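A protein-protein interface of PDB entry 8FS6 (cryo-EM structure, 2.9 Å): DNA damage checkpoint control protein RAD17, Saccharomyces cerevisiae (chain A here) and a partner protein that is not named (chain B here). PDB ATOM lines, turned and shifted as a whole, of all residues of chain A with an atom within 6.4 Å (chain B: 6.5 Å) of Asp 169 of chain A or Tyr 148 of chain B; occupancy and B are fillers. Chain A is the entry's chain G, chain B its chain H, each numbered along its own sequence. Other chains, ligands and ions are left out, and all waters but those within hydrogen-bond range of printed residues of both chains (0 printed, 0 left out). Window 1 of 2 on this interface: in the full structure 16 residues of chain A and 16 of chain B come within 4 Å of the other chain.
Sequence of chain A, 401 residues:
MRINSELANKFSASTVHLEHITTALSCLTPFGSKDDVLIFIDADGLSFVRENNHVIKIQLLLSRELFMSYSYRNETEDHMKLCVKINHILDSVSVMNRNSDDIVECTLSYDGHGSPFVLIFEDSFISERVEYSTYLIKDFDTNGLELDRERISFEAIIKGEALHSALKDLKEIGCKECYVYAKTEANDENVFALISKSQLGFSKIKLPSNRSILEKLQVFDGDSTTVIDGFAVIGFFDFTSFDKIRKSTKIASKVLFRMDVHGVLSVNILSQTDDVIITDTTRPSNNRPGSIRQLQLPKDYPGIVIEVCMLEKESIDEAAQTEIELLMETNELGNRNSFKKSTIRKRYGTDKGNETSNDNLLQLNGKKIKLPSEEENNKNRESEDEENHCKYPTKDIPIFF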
ATOM      1  N   HIS A 164       8.090  10.144 -15.853  1.00  0.00           N
ATOM      2  CA  HIS A 164       7.137  11.249 -15.781  1.00  0.00           C
ATOM      3  C   HIS A 164       5.766  10.763 -15.334  1.00  0.00           C
ATOM      4  O   HIS A 164       5.100  11.420 -14.527  1.00  0.00           O
ATOM      5  CB  HIS A 164       7.041  11.955 -17.134  1.00  0.00           C
ATOM      6  CG  HIS A 164       6.148  13.157 -17.125  1.00  0.00           C
ATOM      7  ND1 HIS A 164       4.830  13.108 -17.526  1.00  0.00           N
ATOM      8  CD2 HIS A 164       6.382  14.440 -16.758  1.00  0.00           C
ATOM      9  CE1 HIS A 164       4.291  14.308 -17.408  1.00  0.00           C
ATOM     10  NE2 HIS A 164       5.211  15.134 -16.944  1.00  0.00           N
ATOM     11  N   SER A 165       5.331   9.607 -15.845  1.00  0.00           N
ATOM     12  CA  SER A 165       4.066   9.032 -15.398  1.00  0.00           C
ATOM     13  C   SER A 165       4.116   8.674 -13.918  1.00  0.00           C
ATOM     14  O   SER A 165       3.133   8.866 -13.191  1.00  0.00           O
ATOM     15  CB  SER A 165       3.723   7.802 -16.237  1.00  0.00           C
ATOM     16  OG  SER A 165       4.731   6.812 -16.125  1.00  0.00           O
ATOM     17  N   ALA A 166       5.254   8.149 -13.455  1.00  0.00           N
ATOM     18  CA  ALA A 166       5.397   7.810 -12.041  1.00  0.00           C
ATOM     19  C   ALA A 166       5.280   9.050 -11.158  1.00  0.00           C
ATOM     20  O   ALA A 166       4.570   9.039 -10.145  1.00  0.00           O
ATOM     21  CB  ALA A 166       6.730   7.102 -11.803  1.00  0.00           C
ATOM     22  N   LEU A 167       5.970  10.133 -11.531  1.00  0.00           N
ATOM     23  CA  LEU A 167       5.870  11.363 -10.742  1.00  0.00           C
ATOM     24  C   LEU A 167       4.472  11.966 -10.810  1.00  0.00           C
ATOM     25  O   LEU A 167       3.988  12.525  -9.819  1.00  0.00           O
ATOM     26  CB  LEU A 167       6.921  12.396 -11.165  1.00  0.00           C
ATOM     27  CG  LEU A 167       8.389  12.199 -10.757  1.00  0.00           C
ATOM     28  CD1 LEU A 167       8.455  11.646  -9.335  1.00  0.00           C
ATOM     29  CD2 LEU A 167       9.240  11.389 -11.711  1.00  0.00           C
ATOM     30  N   LYS A 168       3.808  11.872 -11.965  1.00  0.00           N
ATOM     31  CA  LYS A 168       2.439  12.369 -12.059  1.00  0.00           C
ATOM     32  C   LYS A 168       1.508  11.591 -11.137  1.00  0.00           C
ATOM     33  O   LYS A 168       0.670  12.183 -10.443  1.00  0.00           O
ATOM     34  CB  LYS A 168       1.952  12.296 -13.506  1.00  0.00           C
ATOM     35  CG  LYS A 168       0.760  13.195 -13.803  1.00  0.00           C
ATOM     36  CD  LYS A 168       0.449  13.264 -15.296  1.00  0.00           C
ATOM     37  CE  LYS A 168       0.755  11.954 -16.010  1.00  0.00           C
ATOM     38  NZ  LYS A 168       0.796  12.128 -17.489  1.00  0.00           N
ATOM     39  N   ASP A 169       1.650  10.264 -11.105  1.00  0.00           N
ATOM     40  CA  ASP A 169       0.839   9.454 -10.199  1.00  0.00           C
ATOM     41  C   ASP A 169       1.138   9.789  -8.743  1.00  0.00           C
ATOM     42  O   ASP A 169       0.220   9.876  -7.918  1.00  0.00           O
ATOM     43  CB  ASP A 169       1.077   7.968 -10.466  1.00  0.00           C
ATOM     44  CG  ASP A 169       0.126   7.079  -9.690  1.00  0.00           C
ATOM     45  OD1 ASP A 169      -0.959   7.559  -9.303  1.00  0.00           O
ATOM     46  OD2 ASP A 169       0.466   5.898  -9.464  1.00  0.00           O
ATOM     47  N   LEU A 170       2.418   9.982  -8.409  1.00  0.00           N
ATOM     48  CA  LEU A 170       2.780  10.335  -7.040  1.00  0.00           C
ATOM     49  C   LEU A 170       2.177  11.676  -6.636  1.00  0.00           C
ATOM     50  O   LEU A 170       1.682  11.829  -5.514  1.00  0.00           O
ATOM     51  CB  LEU A 170       4.301  10.363  -6.886  1.00  0.00           C
ATOM     52  CG  LEU A 170       5.016   9.011  -6.922  1.00  0.00           C
ATOM     53  CD1 LEU A 170       6.511   9.186  -6.704  1.00  0.00           C
ATOM     54  CD2 LEU A 170       4.426   8.064  -5.891  1.00  0.00           C
ATOM     55  N   LYS A 171       2.207  12.658  -7.539  1.00  0.00           N
ATOM     56  CA  LYS A 171       1.579  13.944  -7.253  1.00  0.00           C
ATOM     57  C   LYS A 171       0.074  13.792  -7.068  1.00  0.00           C
ATOM     58  O   LYS A 171      -0.514  14.400  -6.165  1.00  0.00           O
ATOM     59  CB  LYS A 171       1.887  14.943  -8.369  1.00  0.00           C
ATOM     60  CG  LYS A 171       0.777  15.953  -8.625  1.00  0.00           C
ATOM     61  CD  LYS A 171       1.283  17.168  -9.378  1.00  0.00           C
ATOM     62  CE  LYS A 171       2.178  18.025  -8.502  1.00  0.00           C
ATOM     63  NZ  LYS A 171       1.478  18.491  -7.273  1.00  0.00           N
ATOM     64  N   GLU A 172      -0.567  12.974  -7.909  1.00  0.00           N
ATOM     65  CA  GLU A 172      -2.012  12.802  -7.806  1.00  0.00           C
ATOM     66  C   GLU A 172      -2.416  12.086  -6.522  1.00  0.00           C
ATOM     67  O   GLU A 172      -3.502  12.345  -5.990  1.00  0.00           O
ATOM     68  CB  GLU A 172      -2.543  12.046  -9.024  1.00  0.00           C
ATOM     69  CG  GLU A 172      -2.480  12.835 -10.321  1.00  0.00           C
ATOM     70  CD  GLU A 172      -3.113  12.098 -11.483  1.00  0.00           C
ATOM     71  OE1 GLU A 172      -4.071  11.331 -11.251  1.00  0.00           O
ATOM     72  OE2 GLU A 172      -2.652  12.284 -12.629  1.00  0.00           O
ATOM     73  N   ILE A 173      -1.571  11.193  -6.006  1.00  0.00           N
ATOM     74  CA  ILE A 173      -1.907  10.464  -4.786  1.00  0.00           C
ATOM     75  C   ILE A 173      -1.371  11.205  -3.566  1.00  0.00           C
ATOM     76  O   ILE A 173      -1.364  10.665  -2.454  1.00  0.00           O
ATOM     77  CB  ILE A 173      -1.378   9.018  -4.827  1.00  0.00           C
ATOM     78  CG1 ILE A 173       0.151   8.999  -4.802  1.00  0.00           C
ATOM     79  CG2 ILE A 173      -1.917   8.285  -6.047  1.00  0.00           C
ATOM     80  CD1 ILE A 173       0.730   7.955  -3.875  1.00  0.00           C
ATOM     81  N   GLY A 174      -0.937  12.447  -3.760  1.00  0.00           N
ATOM     82  CA  GLY A 174      -0.424  13.257  -2.670  1.00  0.00           C
ATOM     83  C   GLY A 174       1.066  13.105  -2.443  1.00  0.00           C
ATOM     84  O   GLY A 174       1.839  14.001  -2.798  1.00  0.00           O
ATOM     85  N   CYS A 175       1.478  11.979  -1.854  1.00  0.00           N
ATOM     86  CA  CYS A 175       2.889  11.628  -1.667  1.00  0.00           C
ATOM     87  C   CYS A 175       3.625  12.710  -0.868  1.00  0.00           C
ATOM     88  O   CYS A 175       4.448  13.461  -1.389  1.00  0.00           O
ATOM     89  CB  CYS A 175       3.573  11.368  -3.015  1.00  0.00           C
ATOM     90  SG  CYS A 175       5.312  10.881  -2.913  1.00  0.00           S
ATOM     91  N   LEU A 200      -3.228   7.940   1.237  1.00  0.00           N
ATOM     92  CA  LEU A 200      -3.716   6.587   0.987  1.00  0.00           C
ATOM     93  C   LEU A 200      -3.045   5.586   1.915  1.00  0.00           C
ATOM     94  O   LEU A 200      -3.689   4.654   2.411  1.00  0.00           O
ATOM     95  CB  LEU A 200      -3.470   6.203  -0.473  1.00  0.00           C
ATOM     96  CG  LEU A 200      -4.555   6.493  -1.514  1.00  0.00           C
ATOM     97  CD1 LEU A 200      -4.967   7.958  -1.514  1.00  0.00           C
ATOM     98  CD2 LEU A 200      -4.066   6.081  -2.890  1.00  0.00           C
ATOM     99  N   PHE A 202       0.556   3.268   2.062  1.00  0.00           N
ATOM    100  CA  PHE A 202       1.820   2.808   1.516  1.00  0.00           C
ATOM    101  C   PHE A 202       1.602   2.414   0.059  1.00  0.00           C
ATOM    102  O   PHE A 202       0.887   1.447  -0.223  1.00  0.00           O
ATOM    103  CB  PHE A 202       2.334   1.630   2.335  1.00  0.00           C
ATOM    104  CG  PHE A 202       3.543   1.949   3.142  1.00  0.00           C
ATOM    105  CD1 PHE A 202       3.429   2.481   4.411  1.00  0.00           C
ATOM    106  CD2 PHE A 202       4.797   1.776   2.624  1.00  0.00           C
ATOM    107  CE1 PHE A 202       4.566   2.789   5.148  1.00  0.00           C
ATOM    108  CE2 PHE A 202       5.907   2.054   3.374  1.00  0.00           C
ATOM    109  CZ  PHE A 202       5.796   2.577   4.619  1.00  0.00           C
ATOM    110  N   SER A 203       2.205   3.165  -0.863  1.00  0.00           N
ATOM    111  CA  SER A 203       2.010   2.953  -2.291  1.00  0.00           C
ATOM    112  C   SER A 203       3.353   2.711  -2.964  1.00  0.00           C
ATOM    113  O   SER A 203       4.354   3.341  -2.611  1.00  0.00           O
ATOM    114  CB  SER A 203       1.306   4.151  -2.942  1.00  0.00           C
ATOM    115  OG  SER A 203       0.062   4.413  -2.318  1.00  0.00           O
ATOM    116  N   LYS A 204       3.371   1.800  -3.935  1.00  0.00           N
ATOM    117  CA  LYS A 204       4.595   1.417  -4.627  1.00  0.00           C
ATOM    118  C   LYS A 204       4.384   1.502  -6.131  1.00  0.00           C
ATOM    119  O   LYS A 204       3.397   0.976  -6.652  1.00  0.00           O
ATOM    120  CB  LYS A 204       5.024  -0.002  -4.236  1.00  0.00           C
ATOM    121  CG  LYS A 204       6.093  -0.602  -5.129  1.00  0.00           C
ATOM    122  CD  LYS A 204       6.360  -2.047  -4.754  1.00  0.00           C
ATOM    123  CE  LYS A 204       5.354  -2.979  -5.404  1.00  0.00           C
ATOM    124  NZ  LYS A 204       6.014  -4.077  -6.162  1.00  0.00           N
ATOM    125  N   ILE A 205       5.312   2.163  -6.823  1.00  0.00           N
ATOM    126  CA  ILE A 205       5.296   2.222  -8.280  1.00  0.00           C
ATOM    127  C   ILE A 205       6.550   1.540  -8.807  1.00  0.00           C
ATOM    128  O   ILE A 205       7.609   2.167  -8.926  1.00  0.00           O
ATOM    129  CB  ILE A 205       5.199   3.672  -8.789  1.00  0.00           C
ATOM    130  CG1 ILE A 205       4.011   4.388  -8.141  1.00  0.00           C
ATOM    131  CG2 ILE A 205       5.076   3.698 -10.306  1.00  0.00           C
ATOM    132  CD1 ILE A 205       3.715   5.746  -8.740  1.00  0.00           C
ATOM    133  N   THR B 103      -9.077   7.751  -6.491  1.00  0.00           N
ATOM    134  CA  THR B 103      -7.800   8.173  -7.048  1.00  0.00           C
ATOM    135  C   THR B 103      -6.920   6.996  -7.444  1.00  0.00           C
ATOM    136  O   THR B 103      -5.844   7.206  -8.016  1.00  0.00           O
ATOM    137  CB  THR B 103      -7.052   9.069  -6.052  1.00  0.00           C
ATOM    138  OG1 THR B 103      -6.092   9.870  -6.753  1.00  0.00           O
ATOM    139  CG2 THR B 103      -6.338   8.235  -4.999  1.00  0.00           C
ATOM    140  N   ILE B 104      -7.352   5.770  -7.158  1.00  0.00           N
ATOM    141  CA  ILE B 104      -6.635   4.576  -7.589  1.00  0.00           C
ATOM    142  C   ILE B 104      -7.203   4.034  -8.894  1.00  0.00           C
ATOM    143  O   ILE B 104      -6.452   3.657  -9.797  1.00  0.00           O
ATOM    144  CB  ILE B 104      -6.675   3.515  -6.472  1.00  0.00           C
ATOM    145  CG1 ILE B 104      -5.962   4.026  -5.221  1.00  0.00           C
ATOM    146  CG2 ILE B 104      -6.048   2.217  -6.940  1.00  0.00           C
ATOM    147  CD1 ILE B 104      -6.035   3.076  -4.047  1.00  0.00           C
ATOM    148  N   ARG B 106      -8.779   5.673 -11.174  1.00  0.00           N
ATOM    149  CA  ARG B 106      -8.782   6.648 -12.255  1.00  0.00           C
ATOM    150  C   ARG B 106      -7.865   6.197 -13.384  1.00  0.00           C
ATOM    151  O   ARG B 106      -6.806   5.606 -13.150  1.00  0.00           O
ATOM    152  CB  ARG B 106      -8.344   8.016 -11.736  1.00  0.00           C
ATOM    153  CG  ARG B 106      -7.059   7.981 -10.928  1.00  0.00           C
ATOM    154  CD  ARG B 106      -5.883   8.531 -11.720  1.00  0.00           C
ATOM    155  NE  ARG B 106      -4.837   9.055 -10.849  1.00  0.00           N
ATOM    156  CZ  ARG B 106      -3.930   8.306 -10.238  1.00  0.00           C
ATOM    157  NH1 ARG B 106      -3.904   6.991 -10.388  1.00  0.00           N
ATOM    158  NH2 ARG B 106      -3.025   8.888  -9.457  1.00  0.00           N
ATOM    159  N   PRO B 108      -5.131   6.828 -15.943  1.00  0.00           N
ATOM    160  CA  PRO B 108      -4.092   7.818 -16.248  1.00  0.00           C
ATOM    161  C   PRO B 108      -4.118   8.206 -17.718  1.00  0.00           C
ATOM    162  O   PRO B 108      -4.421   7.389 -18.592  1.00  0.00           O
ATOM    163  CB  PRO B 108      -2.790   7.096 -15.881  1.00  0.00           C
ATOM    164  CG  PRO B 108      -3.209   5.962 -14.993  1.00  0.00           C
ATOM    165  CD  PRO B 108      -4.557   5.551 -15.491  1.00  0.00           C
ATOM    166  N   LEU B 134      -6.246  -3.027   2.344  1.00  0.00           N
ATOM    167  CA  LEU B 134      -6.726  -3.527   1.064  1.00  0.00           C
ATOM    168  C   LEU B 134      -5.601  -3.494   0.038  1.00  0.00           C
ATOM    169  O   LEU B 134      -4.813  -2.548  -0.010  1.00  0.00           O
ATOM    170  CB  LEU B 134      -7.911  -2.688   0.588  1.00  0.00           C
ATOM    171  CG  LEU B 134      -8.762  -3.217  -0.565  1.00  0.00           C
ATOM    172  CD1 LEU B 134      -9.400  -4.546  -0.199  1.00  0.00           C
ATOM    173  CD2 LEU B 134      -9.826  -2.194  -0.928  1.00  0.00           C
ATOM    174  N   ILE B 135      -5.520  -4.537  -0.783  1.00  0.00           N
ATOM    175  CA  ILE B 135      -4.443  -4.688  -1.757  1.00  0.00           C
ATOM    176  C   ILE B 135      -5.011  -4.439  -3.147  1.00  0.00           C
ATOM    177  O   ILE B 135      -5.901  -5.166  -3.603  1.00  0.00           O
ATOM    178  CB  ILE B 135      -3.787  -6.074  -1.670  1.00  0.00           C
ATOM    179  CG1 ILE B 135      -3.291  -6.339  -0.247  1.00  0.00           C
ATOM    180  CG2 ILE B 135      -2.643  -6.183  -2.664  1.00  0.00           C
ATOM    181  CD1 ILE B 135      -2.653  -7.698  -0.064  1.00  0.00           C
ATOM    182  N   VAL B 136      -4.492  -3.416  -3.821  1.00  0.00           N
ATOM    183  CA  VAL B 136      -4.869  -3.100  -5.194  1.00  0.00           C
ATOM    184  C   VAL B 136      -3.596  -3.047  -6.026  1.00  0.00           C
ATOM    185  O   VAL B 136      -2.679  -2.279  -5.714  1.00  0.00           O
ATOM    186  CB  VAL B 136      -5.636  -1.772  -5.298  1.00  0.00           C
ATOM    187  CG1 VAL B 136      -5.909  -1.436  -6.755  1.00  0.00           C
ATOM    188  CG2 VAL B 136      -6.934  -1.842  -4.510  1.00  0.00           C
ATOM    189  N   VAL B 137      -3.540  -3.856  -7.081  1.00  0.00           N
ATOM    190  CA  VAL B 137      -2.394  -3.916  -7.979  1.00  0.00           C
ATOM    191  C   VAL B 137      -2.856  -3.506  -9.370  1.00  0.00           C
ATOM    192  O   VAL B 137      -3.822  -4.069  -9.898  1.00  0.00           O
ATOM    193  CB  VAL B 137      -1.762  -5.319  -8.005  1.00  0.00           C
ATOM    194  CG1 VAL B 137      -0.546  -5.338  -8.918  1.00  0.00           C
ATOM    195  CG2 VAL B 137      -1.384  -5.757  -6.598  1.00  0.00           C
ATOM    196  N   ILE B 138      -2.169  -2.530  -9.956  1.00  0.00           N
ATOM    197  CA  ILE B 138      -2.500  -2.008 -11.276  1.00  0.00           C
ATOM    198  C   ILE B 138      -1.312  -2.234 -12.198  1.00  0.00           C
ATOM    199  O   ILE B 138      -0.185  -1.841 -11.875  1.00  0.00           O
ATOM    200  CB  ILE B 138      -2.867  -0.514 -11.223  1.00  0.00           C
ATOM    201  CG1 ILE B 138      -3.966  -0.266 -10.190  1.00  0.00           C
ATOM    202  CG2 ILE B 138      -3.301  -0.022 -12.594  1.00  0.00           C
ATOM    203  CD1 ILE B 138      -4.294   1.193 -10.001  1.00  0.00           C
ATOM    204  N   LYS B 146       1.902  -0.672 -10.362  1.00  0.00           N
ATOM    205  CA  LYS B 146       1.599   0.286  -9.305  1.00  0.00           C
ATOM    206  C   LYS B 146       0.705  -0.404  -8.283  1.00  0.00           C
ATOM    207  O   LYS B 146      -0.461  -0.699  -8.569  1.00  0.00           O
ATOM    208  CB  LYS B 146       0.929   1.536  -9.874  1.00  0.00           C
ATOM    209  CG  LYS B 146       1.587   2.077 -11.133  1.00  0.00           C
ATOM    210  CD  LYS B 146       0.986   3.411 -11.553  1.00  0.00           C
ATOM    211  CE  LYS B 146      -0.533   3.394 -11.479  1.00  0.00           C
ATOM    212  NZ  LYS B 146      -1.121   4.717 -11.831  1.00  0.00           N
ATOM    213  N   GLU B 147       1.249  -0.660  -7.098  1.00  0.00           N
ATOM    214  CA  GLU B 147       0.521  -1.318  -6.024  1.00  0.00           C
ATOM    215  C   GLU B 147       0.196  -0.309  -4.931  1.00  0.00           C
ATOM    216  O   GLU B 147       1.050   0.491  -4.534  1.00  0.00           O
ATOM    217  CB  GLU B 147       1.325  -2.492  -5.450  1.00  0.00           C
ATOM    218  CG  GLU B 147       1.259  -2.636  -3.934  1.00  0.00           C
ATOM    219  CD  GLU B 147       1.916  -3.908  -3.436  1.00  0.00           C
ATOM    220  OE1 GLU B 147       1.559  -4.370  -2.331  1.00  0.00           O
ATOM    221  OE2 GLU B 147       2.783  -4.453  -4.149  1.00  0.00           O
ATOM    222  N   TYR B 148      -1.048  -0.342  -4.462  1.00  0.00           N
ATOM    223  CA  TYR B 148      -1.518   0.530  -3.398  1.00  0.00           C
ATOM    224  C   TYR B 148      -2.040  -0.315  -2.245  1.00  0.00           C
ATOM    225  O   TYR B 148      -2.522  -1.434  -2.444  1.00  0.00           O
ATOM    226  CB  TYR B 148      -2.624   1.471  -3.890  1.00  0.00           C
ATOM    227  CG  TYR B 148      -2.239   2.312  -5.084  1.00  0.00           C
ATOM    228  CD1 TYR B 148      -1.642   3.554  -4.920  1.00  0.00           C
ATOM    229  CD2 TYR B 148      -2.477   1.865  -6.377  1.00  0.00           C
ATOM    230  CE1 TYR B 148      -1.290   4.327  -6.008  1.00  0.00           C
ATOM    231  CE2 TYR B 148      -2.129   2.631  -7.473  1.00  0.00           C
ATOM    232  CZ  TYR B 148      -1.536   3.861  -7.282  1.00  0.00           C
ATOM    233  OH  TYR B 148      -1.188   4.625  -8.371  1.00  0.00           O
ATOM    234  N   CYS B 149      -1.942   0.229  -1.036  1.00  0.00           N
ATOM    235  CA  CYS B 149      -2.431  -0.437   0.172  1.00  0.00           C
ATOM    236  C   CYS B 149      -3.295   0.519   0.986  1.00  0.00           C
ATOM    237  O   CYS B 149      -2.886   0.985   2.056  1.00  0.00           O
ATOM    238  CB  CYS B 149      -1.266  -0.969   1.009  1.00  0.00           C
ATOM    239  SG  CYS B 149      -0.423  -2.397   0.291  1.00  0.00           S
ATOM    240  N   PRO B 150      -4.501   0.835   0.508  1.00  0.00           N
ATOM    241  CA  PRO B 150      -5.417   1.632   1.330  1.00  0.00           C
ATOM    242  C   PRO B 150      -5.965   0.811   2.486  1.00  0.00           C
ATOM    243  O   PRO B 150      -6.255  -0.379   2.345  1.00  0.00           O
ATOM    244  CB  PRO B 150      -6.526   2.026   0.348  1.00  0.00           C
ATOM    245  CG  PRO B 150      -6.519   0.940  -0.664  1.00  0.00           C
ATOM    246  CD  PRO B 150      -5.083   0.526  -0.811  1.00  0.00           C
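OD1 of Asp 169 of chain A is in salt-bridge range of NH2 of Arg 106 of chain B, at 2.5 Å.
The side-chain carboxylate (OD2) of Asp 169 of chain A lies within salt-bridge range of the side-chain amino group (NZ) of Lys 146 of chain B (3.1 Å).
The side-chain hydroxyl (OH) of Tyr 148 of chain B sits close to the side-chain carboxylate (OD1) of Asp 169 of chain A (3.1 Å).
OE1 of Glu 172 of chain A is in salt-bridge range of NE of Arg 106 of chain B (2.4 Å).
The backbone NH (N) of Cys 149 of chain B is in hydrogen-bond range of the backbone carbonyl oxygen (O) of Phe 202 of chain A, at 3.2 Å.
OE2 of Glu 147 of chain B is in salt-bridge range of NZ of Lys 204 of chain A (3.8 Å).
O of Thr 103 of chain B lies within hydrogen-bond range of NH1 of Arg 106 of chain B, 3.1 Å away.
The backbone carbonyl oxygen (O) of Pro 150 of chain B lies within hydrogen-bond range of the backbone NH (N) of Leu 134 of chain B.
O of Val 136 of chain B is in hydrogen-bond range of N of Tyr 148 of chain B.
N of Lys 146 of chain B sits at hydrogen-bond distance from O of Ile 138 of chain B, 2.8 Å away.
The side-chain hydroxyl (OH) of Tyr 148 of chain B lies close to the side-chain amino group (NZ) of Lys 146 of chain B (3.5 Å).
Among the printed residues, pairs that only touch across the chains: Ser 203 of chain A with Tyr 148 of chain B, Lys 204 of chain A with Lys 146 of chain B, Ser 203 of chain A with Glu 147 of chain B, Ile 173 of chain A with Arg 106 of chain B, Leu 200 of chain A with Ile 104 of chain B, Leu 200 of chain A with Pro 150 of chain B, Glu 172 of chain A with Thr 103 of chain B, Leu 200 of chain A with Thr 103 of chain B, Leu 200 of chain A with Cys 149 of chain B, Ile 205 of chain A with Lys 146 of chain B and Phe 202 of chain A with Tyr 148 of chain B.
Of chain B, only Arg 106, Lys 146 and Tyr 148 come within 4 Å of Asp 169 of chain A.
Printed residues of chain A within 4 Å of Tyr 148 of chain B: Asp 169 (2.4 Å), Phe 202 (3.97 Å) and Ser 203 (3.2 Å).
Printed residues of chain B within 4 Å of Ile 173 of chain A: Arg 106.
Printed residues of chain B within 4 Å of Lys 204 of chain A: Lys 146 (3.3 Å) and Glu 147 (2.7 Å).
Of the printed residues of chain B, Glu 172 of chain A touches Thr 103 (3.7 Å) and Arg 106 (2.4 Å).
Ile 138 of chain B touches none of the printed residues of chain A.
The nearest residue of chain B that does not touch Asp 169 of chain A is Thr 103 of chain B (5.1 Å).
The nearest printed residue of chain A that does not touch Tyr 148 of chain B is Ile 173 of chain A (4.01 Å).
Of the 17 printed residues of chain A, 8 touch a printed residue of chain B.
Along chain A the printed residues that touch a printed residue of chain B span positions 169 to 205.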
